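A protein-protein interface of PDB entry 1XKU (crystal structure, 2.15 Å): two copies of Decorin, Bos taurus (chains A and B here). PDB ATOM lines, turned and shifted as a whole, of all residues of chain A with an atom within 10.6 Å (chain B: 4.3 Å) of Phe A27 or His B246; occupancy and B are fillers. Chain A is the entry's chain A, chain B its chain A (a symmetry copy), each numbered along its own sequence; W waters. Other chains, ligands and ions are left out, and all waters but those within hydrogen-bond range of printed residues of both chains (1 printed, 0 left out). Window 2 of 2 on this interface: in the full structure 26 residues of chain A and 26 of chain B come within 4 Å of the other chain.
O of Arg A28 is in hydrogen-bond range of NE2 of Gln A30.
The guanidinium group of Arg A28 lies within hydrogen-bond range of the backbone carbonyl oxygen of Leu A41.
The side-chain amino group (NZ) of Lys B220 lies within salt-bridge range of the side-chain carboxylate (OE1) of Glu B244 (2.9 Å).
The backbone NH (N) of Leu B221 is in hydrogen-bond range of the backbone carbonyl oxygen (O) of Glu B244 (3.0 Å).
The backbone carbonyl oxygen of His B246 is in hydrogen-bond range of the backbone NH of Leu B223, at 2.9 Å.
The side-chain carboxylate (OE2) of Glu B244 sits at hydrogen-bond distance from a ring nitrogen (NE2) of His B246, at 3.4 Å.
Phe A27 touches just these residues of chain B: His B198 (3.5 Å), Lys B220 (3.9 Å), Gly B222 (3.8 Å), Glu B244 (3.6 Å) and His B246 (3.4 Å).
His B246 touches just one residue of chain A: Phe A27 (3.4 Å).
Leu B223 touches none of the printed residues of chain A.
No residue of chain A comes within 4 Å of Ser B224.
Of chain A, only Phe A27 (3.6 Å) comes within 4 Å of Glu B244.
No residue of chain A comes within 4 Å of Leu B245.
No residue of chain A comes within 4 Å of Asn B248.
No residue of chain A comes within 4 Å of Tyr B269.
Of the printed residues of chain B, Arg A28 touches His B198 (3.4 Å).
Printed residues of chain A within 4 Å of His B198: Phe A27 (3.5 Å) and Arg A28 (3.4 Å).
Cys A29 touches none of the printed residues of chain B.
The nearest residue of chain B that does not touch Phe A27 is Leu B221 (4.1 Å).
The nearest residue of chain A that does not touch His B246 is Arg A28 (7.0 Å).
Water W1 lies within hydrogen-bond range of the side-chain amino group (NZ) of Lys B220 (2.7 Å), the backbone carbonyl oxygen (O) of Cys A25 (3.0 Å) and the backbone carbonyl oxygen (O) of Pro A26 (3.5 Å).
No position is printed for both chains.
Of the 6 pairs that touch across the chains among the printed residues, none has its exchanged pair printed and touching as well.
Printed residues of chain B that touch a printed residue of chain A: His B198, Lys B220, Gly B222, Glu B244 and His B246.
Hydrophobic or aromatic side chains of chain B within 4 Å of the printed part of chain A: His B198 and His B246.
Among the printed residues, 6 pairs touch across the chains.
Among the printed residues, pairs that only touch across the chains: Phe A27 with His B198 (3.5 Å), Phe A27 with Lys B220 (3.9 Å), Phe A27 with Gly B222 (3.8 Å), Phe A27 with Glu B244 (3.6 Å), Phe A27 with His B246 (3.4 Å) and Arg A28 with His B198 (3.4 Å).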
ATOM      1  N   PRO A  23      23.624  -2.520 -26.842  1.00  0.00           N
ATOM      2  CA  PRO A  23      24.231  -2.320 -25.527  1.00  0.00           C
ATOM      3  C   PRO A  23      23.366  -1.447 -24.606  1.00  0.00           C
ATOM      4  O   PRO A  23      22.480  -0.725 -25.073  1.00  0.00           O
ATOM      5  CB  PRO A  23      25.572  -1.660 -25.844  1.00  0.00           C
ATOM      6  CG  PRO A  23      25.326  -0.919 -27.098  1.00  0.00           C
ATOM      7  CD  PRO A  23      24.262  -1.681 -27.871  1.00  0.00           C
ATOM      8  N   VAL A  24      23.623  -1.546 -23.309  1.00  0.00           N
ATOM      9  CA  VAL A  24      22.806  -0.881 -22.317  1.00  0.00           C
ATOM     10  C   VAL A  24      23.742  -0.036 -21.437  1.00  0.00           C
ATOM     11  O   VAL A  24      24.823  -0.506 -21.044  1.00  0.00           O
ATOM     12  CB  VAL A  24      22.016  -1.937 -21.470  1.00  0.00           C
ATOM     13  CG1 VAL A  24      21.490  -1.367 -20.159  1.00  0.00           C
ATOM     14  CG2 VAL A  24      20.878  -2.533 -22.258  1.00  0.00           C
ATOM     15  N   CYS A  25      23.309   1.198 -21.149  1.00  0.00           N
ATOM     16  CA  CYS A  25      23.864   2.022 -20.115  1.00  0.00           C
ATOM     17  C   CYS A  25      23.138   1.731 -18.801  1.00  0.00           C
ATOM     18  O   CYS A  25      21.914   1.919 -18.746  1.00  0.00           O
ATOM     19  CB  CYS A  25      23.708   3.492 -20.483  1.00  0.00           C
ATOM     20  SG  CYS A  25      24.757   4.517 -19.432  1.00  0.00           S
ATOM     21  N   PRO A  26      23.850   1.255 -17.756  1.00  0.00           N
ATOM     22  CA  PRO A  26      23.175   0.874 -16.490  1.00  0.00           C
ATOM     23  C   PRO A  26      22.528   2.107 -15.846  1.00  0.00           C
ATOM     24  O   PRO A  26      23.015   3.227 -15.993  1.00  0.00           O
ATOM     25  CB  PRO A  26      24.308   0.288 -15.627  1.00  0.00           C
ATOM     26  CG  PRO A  26      25.417  -0.078 -16.630  1.00  0.00           C
ATOM     27  CD  PRO A  26      25.305   1.016 -17.687  1.00  0.00           C
ATOM     28  N   PHE A  27      21.389   1.890 -15.213  1.00  0.00           N
ATOM     29  CA  PHE A  27      20.594   2.975 -14.642  1.00  0.00           C
ATOM     30  C   PHE A  27      21.440   3.745 -13.655  1.00  0.00           C
ATOM     31  O   PHE A  27      22.052   3.135 -12.737  1.00  0.00           O
ATOM     32  CB  PHE A  27      19.345   2.398 -13.939  1.00  0.00           C
ATOM     33  CG  PHE A  27      18.272   3.400 -13.658  1.00  0.00           C
ATOM     34  CD1 PHE A  27      18.036   3.830 -12.325  1.00  0.00           C
ATOM     35  CD2 PHE A  27      17.431   3.848 -14.700  1.00  0.00           C
ATOM     36  CE1 PHE A  27      16.982   4.786 -12.048  1.00  0.00           C
ATOM     37  CE2 PHE A  27      16.346   4.758 -14.438  1.00  0.00           C
ATOM     38  CZ  PHE A  27      16.157   5.245 -13.095  1.00  0.00           C
ATOM     39  N   ARG A  28      21.478   5.079 -13.885  1.00  0.00           N
ATOM     40  CA  ARG A  28      22.247   6.070 -13.132  1.00  0.00           C
ATOM     41  C   ARG A  28      23.611   6.325 -13.682  1.00  0.00           C
ATOM     42  O   ARG A  28      24.197   7.335 -13.362  1.00  0.00           O
ATOM     43  CB  ARG A  28      22.360   5.756 -11.621  1.00  0.00           C
ATOM     44  CG  ARG A  28      21.035   5.731 -10.837  1.00  0.00           C
ATOM     45  CD  ARG A  28      21.155   5.116  -9.449  1.00  0.00           C
ATOM     46  NE  ARG A  28      21.707   3.774  -9.540  1.00  0.00           N
ATOM     47  CZ  ARG A  28      22.240   3.111  -8.513  1.00  0.00           C
ATOM     48  NH1 ARG A  28      22.246   3.654  -7.300  1.00  0.00           N
ATOM     49  NH2 ARG A  28      22.762   1.900  -8.707  1.00  0.00           N
ATOM     50  N   CYS A  29      24.151   5.410 -14.485  1.00  0.00           N
ATOM     51  CA  CYS A  29      25.431   5.664 -15.134  1.00  0.00           C
ATOM     52  C   CYS A  29      25.197   6.652 -16.310  1.00  0.00           C
ATOM     53  O   CYS A  29      24.087   6.813 -16.796  1.00  0.00           O
ATOM     54  CB  CYS A  29      26.034   4.356 -15.711  1.00  0.00           C
ATOM     55  SG  CYS A  29      26.424   3.042 -14.559  1.00  0.00           S
ATOM     56  N   GLN A  30      26.278   7.228 -16.805  1.00  0.00           N
ATOM     57  CA  GLN A  30      26.231   8.143 -17.955  1.00  0.00           C
ATOM     58  C   GLN A  30      27.160   7.533 -18.969  1.00  0.00           C
ATOM     59  O   GLN A  30      28.324   7.250 -18.633  1.00  0.00           O
ATOM     60  CB  GLN A  30      26.729   9.551 -17.512  1.00  0.00           C
ATOM     61  CG  GLN A  30      26.091  10.045 -16.167  1.00  0.00           C
ATOM     62  CD  GLN A  30      26.966   9.859 -14.860  1.00  0.00           C
ATOM     63  OE1 GLN A  30      27.987  10.515 -14.697  1.00  0.00           O
ATOM     64  NE2 GLN A  30      26.526   8.996 -13.946  1.00  0.00           N
ATOM     65  N   CYS A  31      26.654   7.288 -20.176  1.00  0.00           N
ATOM     66  CA  CYS A  31      27.429   6.674 -21.260  1.00  0.00           C
ATOM     67  C   CYS A  31      27.436   7.637 -22.438  1.00  0.00           C
ATOM     68  O   CYS A  31      26.432   7.846 -23.088  1.00  0.00           O
ATOM     69  CB  CYS A  31      26.884   5.279 -21.651  1.00  0.00           C
ATOM     70  SG  CYS A  31      26.621   4.141 -20.218  1.00  0.00           S
ATOM     71  N   VAL A  36      32.100   5.327 -20.105  1.00  0.00           N
ATOM     72  CA  VAL A  36      31.023   4.786 -19.248  1.00  0.00           C
ATOM     73  C   VAL A  36      31.356   5.261 -17.817  1.00  0.00           C
ATOM     74  O   VAL A  36      32.386   4.883 -17.205  1.00  0.00           O
ATOM     75  CB  VAL A  36      30.834   3.204 -19.403  1.00  0.00           C
ATOM     76  CG1 VAL A  36      29.932   2.627 -18.323  1.00  0.00           C
ATOM     77  CG2 VAL A  36      30.293   2.822 -20.784  1.00  0.00           C
ATOM     78  N   GLN A  37      30.542   6.211 -17.345  1.00  0.00           N
ATOM     79  CA  GLN A  37      30.727   6.784 -16.018  1.00  0.00           C
ATOM     80  C   GLN A  37      29.722   6.131 -15.044  1.00  0.00           C
ATOM     81  O   GLN A  37      28.544   6.476 -15.054  1.00  0.00           O
ATOM     82  CB  GLN A  37      30.606   8.334 -16.069  1.00  0.00           C
ATOM     83  CG  GLN A  37      30.707   8.982 -14.665  1.00  0.00           C
ATOM     84  CD  GLN A  37      31.978   8.595 -13.913  1.00  0.00           C
ATOM     85  OE1 GLN A  37      31.944   7.707 -13.073  1.00  0.00           O
ATOM     86  NE2 GLN A  37      33.095   9.266 -14.210  1.00  0.00           N
ATOM     87  N   CYS A  38      30.202   5.209 -14.194  1.00  0.00           N
ATOM     88  CA  CYS A  38      29.396   4.542 -13.170  1.00  0.00           C
ATOM     89  C   CYS A  38      29.832   4.740 -11.725  1.00  0.00           C
ATOM     90  O   CYS A  38      29.489   3.931 -10.881  1.00  0.00           O
ATOM     91  CB  CYS A  38      29.345   3.022 -13.495  1.00  0.00           C
ATOM     92  SG  CYS A  38      28.412   2.529 -14.945  1.00  0.00           S
ATOM     93  N   SER A  39      30.651   5.747 -11.431  1.00  0.00           N
ATOM     94  CA  SER A  39      31.126   6.053 -10.070  1.00  0.00           C
ATOM     95  C   SER A  39      29.951   6.305  -9.155  1.00  0.00           C
ATOM     96  O   SER A  39      28.981   6.899  -9.612  1.00  0.00           O
ATOM     97  CB  SER A  39      31.872   7.419 -10.008  1.00  0.00           C
ATOM     98  OG  SER A  39      33.069   7.288 -10.629  1.00  0.00           O
ATOM     99  N   ASP A  40      30.137   5.981  -7.862  1.00  0.00           N
ATOM    100  CA  ASP A  40      29.311   6.464  -6.725  1.00  0.00           C
ATOM    101  C   ASP A  40      27.903   5.877  -6.660  1.00  0.00           C
ATOM    102  O   ASP A  40      26.958   6.522  -6.154  1.00  0.00           O
ATOM    103  CB  ASP A  40      29.219   8.007  -6.647  1.00  0.00           C
ATOM    104  CG  ASP A  40      30.557   8.714  -6.837  1.00  0.00           C
ATOM    105  OD1 ASP A  40      30.632   9.691  -7.653  1.00  0.00           O
ATOM    106  OD2 ASP A  40      31.571   8.372  -6.232  1.00  0.00           O
ATOM    107  N   LEU A  41      27.755   4.671  -7.195  1.00  0.00           N
ATOM    108  CA  LEU A  41      26.429   4.075  -7.316  1.00  0.00           C
ATOM    109  C   LEU A  41      26.178   2.903  -6.409  1.00  0.00           C
ATOM    110  O   LEU A  41      25.135   2.330  -6.500  1.00  0.00           O
ATOM    111  CB  LEU A  41      26.140   3.660  -8.768  1.00  0.00           C
ATOM    112  CG  LEU A  41      26.241   4.829  -9.782  1.00  0.00           C
ATOM    113  CD1 LEU A  41      26.031   4.306 -11.199  1.00  0.00           C
ATOM    114  CD2 LEU A  41      25.215   6.003  -9.466  1.00  0.00           C
ATOM    115  N   GLY A  42      27.122   2.529  -5.554  1.00  0.00           N
ATOM    116  CA  GLY A  42      26.967   1.328  -4.751  1.00  0.00           C
ATOM    117  C   GLY A  42      26.816   0.045  -5.560  1.00  0.00           C
ATOM    118  O   GLY A  42      26.249  -0.914  -5.071  1.00  0.00           O
ATOM    119  N   LEU A  43      27.324  -0.018  -6.791  1.00  0.00           N
ATOM    120  CA  LEU A  43      27.179  -1.251  -7.586  1.00  0.00           C
ATOM    121  C   LEU A  43      27.918  -2.405  -6.929  1.00  0.00           C
ATOM    122  O   LEU A  43      28.979  -2.185  -6.301  1.00  0.00           O
ATOM    123  CB  LEU A  43      27.696  -1.029  -8.993  1.00  0.00           C
ATOM    124  CG  LEU A  43      27.009   0.060  -9.835  1.00  0.00           C
ATOM    125  CD1 LEU A  43      27.790   0.177 -11.105  1.00  0.00           C
ATOM    126  CD2 LEU A  43      25.604  -0.376 -10.151  1.00  0.00           C
ATOM    127  N   GLU A  44      27.394  -3.631  -7.075  1.00  0.00           N
ATOM    128  CA  GLU A  44      27.999  -4.783  -6.413  1.00  0.00           C
ATOM    129  C   GLU A  44      28.760  -5.684  -7.354  1.00  0.00           C
ATOM    130  O   GLU A  44      29.449  -6.553  -6.913  1.00  0.00           O
ATOM    131  CB  GLU A  44      26.948  -5.581  -5.617  1.00  0.00           C
ATOM    132  CG  GLU A  44      26.370  -4.791  -4.451  1.00  0.00           C
ATOM    133  CD  GLU A  44      25.117  -5.433  -3.837  1.00  0.00           C
ATOM    134  OE1 GLU A  44      24.721  -5.006  -2.724  1.00  0.00           O
ATOM    135  OE2 GLU A  44      24.511  -6.348  -4.429  1.00  0.00           O
ATOM    136  N   LYS A  45      28.643  -5.470  -8.654  1.00  0.00           N
ATOM    137  CA  LYS A  45      29.459  -6.185  -9.619  1.00  0.00           C
ATOM    138  C   LYS A  45      29.627  -5.341 -10.858  1.00  0.00           C
ATOM    139  O   LYS A  45      28.985  -4.307 -11.004  1.00  0.00           O
ATOM    140  CB  LYS A  45      28.885  -7.586  -9.932  1.00  0.00           C
ATOM    141  CG  LYS A  45      27.469  -7.586 -10.438  1.00  0.00           C
ATOM    142  CD  LYS A  45      26.681  -8.729  -9.827  1.00  0.00           C
ATOM    143  CE  LYS A  45      27.106 -10.075 -10.438  1.00  0.00           C
ATOM    144  NZ  LYS A  45      26.996 -11.183  -9.450  1.00  0.00           N
ATOM    145  N   PRO A  47      29.093  -4.121 -14.413  1.00  0.00           N
ATOM    146  CA  PRO A  47      27.966  -4.179 -15.331  1.00  0.00           C
ATOM    147  C   PRO A  47      28.368  -4.926 -16.616  1.00  0.00           C
ATOM    148  O   PRO A  47      29.495  -4.763 -17.089  1.00  0.00           O
ATOM    149  CB  PRO A  47      27.667  -2.697 -15.663  1.00  0.00           C
ATOM    150  CG  PRO A  47      28.547  -1.826 -14.813  1.00  0.00           C
ATOM    151  CD  PRO A  47      29.560  -2.740 -14.126  1.00  0.00           C
ATOM    152  N   LYS A  48      27.450  -5.707 -17.165  1.00  0.00           N
ATOM    153  CA  LYS A  48      27.628  -6.355 -18.453  1.00  0.00           C
ATOM    154  C   LYS A  48      26.884  -5.613 -19.573  1.00  0.00           C
ATOM    155  O   LYS A  48      26.140  -4.653 -19.309  1.00  0.00           O
ATOM    156  CB  LYS A  48      27.201  -7.823 -18.349  1.00  0.00           C
ATOM    157  CG  LYS A  48      28.296  -8.684 -17.637  1.00  0.00           C
ATOM    158  CD  LYS A  48      28.100 -10.181 -17.900  1.00  0.00           C
ATOM    159  CE  LYS A  48      28.895 -11.018 -16.928  1.00  0.00           C
ATOM    160  NZ  LYS A  48      28.922 -12.491 -17.350  1.00  0.00           N
ATOM    161  N   ASP A  49      27.099  -6.033 -20.828  1.00  0.00           N
ATOM    162  CA  ASP A  49      26.393  -5.432 -21.975  1.00  0.00           C
ATOM    163  C   ASP A  49      26.676  -3.950 -22.204  1.00  0.00           C
ATOM    164  O   ASP A  49      25.797  -3.234 -22.696  1.00  0.00           O
ATOM    165  CB  ASP A  49      24.871  -5.580 -21.808  1.00  0.00           C
ATOM    166  CG  ASP A  49      24.437  -7.019 -21.687  1.00  0.00           C
ATOM    167  OD1 ASP A  49      24.870  -7.855 -22.522  1.00  0.00           O
ATOM    168  OD2 ASP A  49      23.676  -7.407 -20.761  1.00  0.00           O
ATOM    169  N   LEU A  50      27.876  -3.489 -21.846  1.00  0.00           N
ATOM    170  CA  LEU A  50      28.253  -2.117 -22.076  1.00  0.00           C
ATOM    171  C   LEU A  50      28.556  -1.943 -23.560  1.00  0.00           C
ATOM    172  O   LEU A  50      28.918  -2.913 -24.201  1.00  0.00           O
ATOM    173  CB  LEU A  50      29.468  -1.765 -21.218  1.00  0.00           C
ATOM    174  CG  LEU A  50      29.265  -1.776 -19.690  1.00  0.00           C
ATOM    175  CD1 LEU A  50      30.581  -1.512 -19.050  1.00  0.00           C
ATOM    176  CD2 LEU A  50      28.191  -0.757 -19.202  1.00  0.00           C
ATOM    177  N   LEU A  59      34.444   2.862 -12.623  1.00  0.00           N
ATOM    178  CA  LEU A  59      33.672   2.174 -11.613  1.00  0.00           C
ATOM    179  C   LEU A  59      34.106   2.525 -10.191  1.00  0.00           C
ATOM    180  O   LEU A  59      33.841   1.787  -9.273  1.00  0.00           O
ATOM    181  CB  LEU A  59      33.721   0.648 -11.832  1.00  0.00           C
ATOM    182  CG  LEU A  59      32.848   0.108 -13.007  1.00  0.00           C
ATOM    183  CD1 LEU A  59      33.300  -1.282 -13.515  1.00  0.00           C
ATOM    184  CD2 LEU A  59      31.310   0.182 -12.657  1.00  0.00           C
ATOM    185  N   ASN A  62      32.336   2.068  -5.707  1.00  0.00           N
ATOM    186  CA  ASN A  62      31.163   1.220  -5.685  1.00  0.00           C
ATOM    187  C   ASN A  62      31.471   0.133  -4.641  1.00  0.00           C
ATOM    188  O   ASN A  62      32.390   0.333  -3.802  1.00  0.00           O
ATOM    189  CB  ASN A  62      30.892   0.658  -7.091  1.00  0.00           C
ATOM    190  CG  ASN A  62      30.282   1.666  -8.012  1.00  0.00           C
ATOM    191  OD1 ASN A  62      29.148   2.090  -7.799  1.00  0.00           O
ATOM    192  ND2 ASN A  62      31.035   2.108  -9.041  1.00  0.00           N
ATOM    193  N   HIS B 198      17.855  11.564 -10.883  1.00  0.00           N
ATOM    194  CA  HIS B 198      18.165  10.473 -10.011  1.00  0.00           C
ATOM    195  C   HIS B 198      18.203  10.979  -8.622  1.00  0.00           C
ATOM    196  O   HIS B 198      19.014  11.851  -8.257  1.00  0.00           O
ATOM    197  CB  HIS B 198      19.488   9.740 -10.396  1.00  0.00           C
ATOM    198  CG  HIS B 198      19.402   9.061 -11.724  1.00  0.00           C
ATOM    199  ND1 HIS B 198      18.670   7.899 -11.924  1.00  0.00           N
ATOM    200  CD2 HIS B 198      19.845   9.453 -12.949  1.00  0.00           C
ATOM    201  CE1 HIS B 198      18.746   7.566 -13.201  1.00  0.00           C
ATOM    202  NE2 HIS B 198      19.467   8.487 -13.842  1.00  0.00           N
ATOM    203  N   LYS B 220      14.131   9.421 -17.768  1.00  0.00           N
ATOM    204  CA  LYS B 220      14.308   8.546 -16.606  1.00  0.00           C
ATOM    205  C   LYS B 220      14.110   9.300 -15.310  1.00  0.00           C
ATOM    206  O   LYS B 220      14.625  10.419 -15.160  1.00  0.00           O
ATOM    207  CB  LYS B 220      15.693   7.894 -16.617  1.00  0.00           C
ATOM    208  CG  LYS B 220      16.070   7.166 -17.914  1.00  0.00           C
ATOM    209  CD  LYS B 220      17.435   6.548 -17.803  1.00  0.00           C
ATOM    210  CE  LYS B 220      17.984   6.138 -19.192  1.00  0.00           C
ATOM    211  NZ  LYS B 220      18.093   4.661 -19.254  1.00  0.00           N
ATOM    212  N   LEU B 221      13.419   8.650 -14.376  1.00  0.00           N
ATOM    213  CA  LEU B 221      13.079   9.199 -13.092  1.00  0.00           C
ATOM    214  C   LEU B 221      13.391   8.127 -12.025  1.00  0.00           C
ATOM    215  O   LEU B 221      12.712   7.112 -11.929  1.00  0.00           O
ATOM    216  CB  LEU B 221      11.572   9.671 -13.037  1.00  0.00           C
ATOM    217  CG  LEU B 221      11.059  10.308 -11.719  1.00  0.00           C
ATOM    218  CD1 LEU B 221      12.076  11.353 -11.110  1.00  0.00           C
ATOM    219  CD2 LEU B 221       9.615  10.908 -11.850  1.00  0.00           C
ATOM    220  N   GLY B 222      14.481   8.328 -11.287  1.00  0.00           N
ATOM    221  CA  GLY B 222      14.871   7.375 -10.260  1.00  0.00           C
ATOM    222  C   GLY B 222      14.503   7.884  -8.882  1.00  0.00           C
ATOM    223  O   GLY B 222      15.032   8.915  -8.408  1.00  0.00           O
ATOM    224  N   LEU B 223      13.545   7.195  -8.261  1.00  0.00           N
ATOM    225  CA  LEU B 223      13.012   7.577  -6.935  1.00  0.00           C
ATOM    226  C   LEU B 223      13.072   6.396  -5.981  1.00  0.00           C
ATOM    227  O   LEU B 223      12.391   6.359  -4.942  1.00  0.00           O
ATOM    228  CB  LEU B 223      11.563   8.086  -7.082  1.00  0.00           C
ATOM    229  CG  LEU B 223      11.402   9.474  -7.744  1.00  0.00           C
ATOM    230  CD1 LEU B 223       9.905   9.752  -8.074  1.00  0.00           C
ATOM    231  CD2 LEU B 223      11.914  10.543  -6.785  1.00  0.00           C
ATOM    232  N   SER B 224      13.927   5.437  -6.312  1.00  0.00           N
ATOM    233  CA  SER B 224      14.064   4.267  -5.503  1.00  0.00           C
ATOM    234  C   SER B 224      14.627   4.559  -4.065  1.00  0.00           C
ATOM    235  O   SER B 224      15.358   5.544  -3.840  1.00  0.00           O
ATOM    236  CB  SER B 224      14.859   3.208  -6.261  1.00  0.00           C
ATOM    237  OG  SER B 224      16.262   3.426  -6.096  1.00  0.00           O
ATOM    238  N   GLU B 244      11.218   5.491 -18.162  1.00  0.00           N
ATOM    239  CA  GLU B 244      11.586   4.606 -17.040  1.00  0.00           C
ATOM    240  C   GLU B 244      11.335   5.232 -15.723  1.00  0.00           C
ATOM    241  O   GLU B 244      11.846   6.315 -15.433  1.00  0.00           O
ATOM    242  CB  GLU B 244      13.059   4.179 -17.007  1.00  0.00           C
ATOM    243  CG  GLU B 244      13.637   3.678 -18.277  1.00  0.00           C
ATOM    244  CD  GLU B 244      14.980   2.926 -18.003  1.00  0.00           C
ATOM    245  OE1 GLU B 244      15.794   3.012 -18.898  1.00  0.00           O
ATOM    246  OE2 GLU B 244      15.181   2.208 -16.944  1.00  0.00           O
ATOM    247  N   LEU B 245      10.627   4.501 -14.875  1.00  0.00           N
ATOM    248  CA  LEU B 245      10.224   5.022 -13.584  1.00  0.00           C
ATOM    249  C   LEU B 245      10.558   3.965 -12.520  1.00  0.00           C
ATOM    250  O   LEU B 245       9.975   2.893 -12.500  1.00  0.00           O
ATOM    251  CB  LEU B 245       8.708   5.355 -13.608  1.00  0.00           C
ATOM    252  CG  LEU B 245       8.017   5.742 -12.287  1.00  0.00           C
ATOM    253  CD1 LEU B 245       8.659   6.982 -11.601  1.00  0.00           C
ATOM    254  CD2 LEU B 245       6.516   5.946 -12.532  1.00  0.00           C
ATOM    255  N   HIS B 246      11.538   4.273 -11.667  1.00  0.00           N
ATOM    256  CA  HIS B 246      11.920   3.375 -10.610  1.00  0.00           C
ATOM    257  C   HIS B 246      11.379   3.920  -9.313  1.00  0.00           C
ATOM    258  O   HIS B 246      11.841   4.938  -8.809  1.00  0.00           O
ATOM    259  CB  HIS B 246      13.432   3.186 -10.477  1.00  0.00           C
ATOM    260  CG  HIS B 246      14.090   2.565 -11.666  1.00  0.00           C
ATOM    261  ND1 HIS B 246      15.237   1.810 -11.550  1.00  0.00           N
ATOM    262  CD2 HIS B 246      13.768   2.563 -12.985  1.00  0.00           C
ATOM    263  CE1 HIS B 246      15.608   1.389 -12.745  1.00  0.00           C
ATOM    264  NE2 HIS B 246      14.740   1.844 -13.636  1.00  0.00           N
ATOM    265  N   LEU B 247      10.419   3.206  -8.753  1.00  0.00           N
ATOM    266  CA  LEU B 247       9.814   3.621  -7.509  1.00  0.00           C
ATOM    267  C   LEU B 247       9.873   2.473  -6.467  1.00  0.00           C
ATOM    268  O   LEU B 247       9.219   2.525  -5.444  1.00  0.00           O
ATOM    269  CB  LEU B 247       8.395   4.120  -7.791  1.00  0.00           C
ATOM    270  CG  LEU B 247       8.112   5.615  -8.018  1.00  0.00           C
ATOM    271  CD1 LEU B 247       6.655   5.787  -8.466  1.00  0.00           C
ATOM    272  CD2 LEU B 247       8.346   6.398  -6.713  1.00  0.00           C
ATOM    273  N   ASN B 248      10.703   1.456  -6.725  1.00  0.00           N
ATOM    274  CA  ASN B 248      10.854   0.358  -5.766  1.00  0.00           C
ATOM    275  C   ASN B 248      11.384   0.853  -4.417  1.00  0.00           C
ATOM    276  O   ASN B 248      12.062   1.903  -4.376  1.00  0.00           O
ATOM    277  CB  ASN B 248      11.798  -0.720  -6.317  1.00  0.00           C
ATOM    278  CG  ASN B 248      13.170  -0.150  -6.738  1.00  0.00           C
ATOM    279  OD1 ASN B 248      13.285   0.474  -7.793  1.00  0.00           O
ATOM    280  ND2 ASN B 248      14.199  -0.394  -5.942  1.00  0.00           N
ATOM    281  N   TYR B 269       9.129   0.185 -12.093  1.00  0.00           N
ATOM    282  CA  TYR B 269       9.534  -0.642 -10.950  1.00  0.00           C
ATOM    283  C   TYR B 269       8.828  -0.262  -9.679  1.00  0.00           C
ATOM    284  O   TYR B 269       8.932   0.868  -9.182  1.00  0.00           O
ATOM    285  CB  TYR B 269      11.067  -0.632 -10.753  1.00  0.00           C
ATOM    286  CG  TYR B 269      11.815  -1.303 -11.875  1.00  0.00           C
ATOM    287  CD1 TYR B 269      13.138  -0.978 -12.150  1.00  0.00           C
ATOM    288  CD2 TYR B 269      11.200  -2.265 -12.670  1.00  0.00           C
ATOM    289  CE1 TYR B 269      13.836  -1.610 -13.190  1.00  0.00           C
ATOM    290  CE2 TYR B 269      11.877  -2.909 -13.681  1.00  0.00           C
ATOM    291  CZ  TYR B 269      13.192  -2.560 -13.940  1.00  0.00           C
ATOM    292  OH  TYR B 269      13.850  -3.177 -14.957  1.00  0.00           O
HETATM  293  O   HOH W   1      20.524   4.484 -18.066  1.00  0.00           O
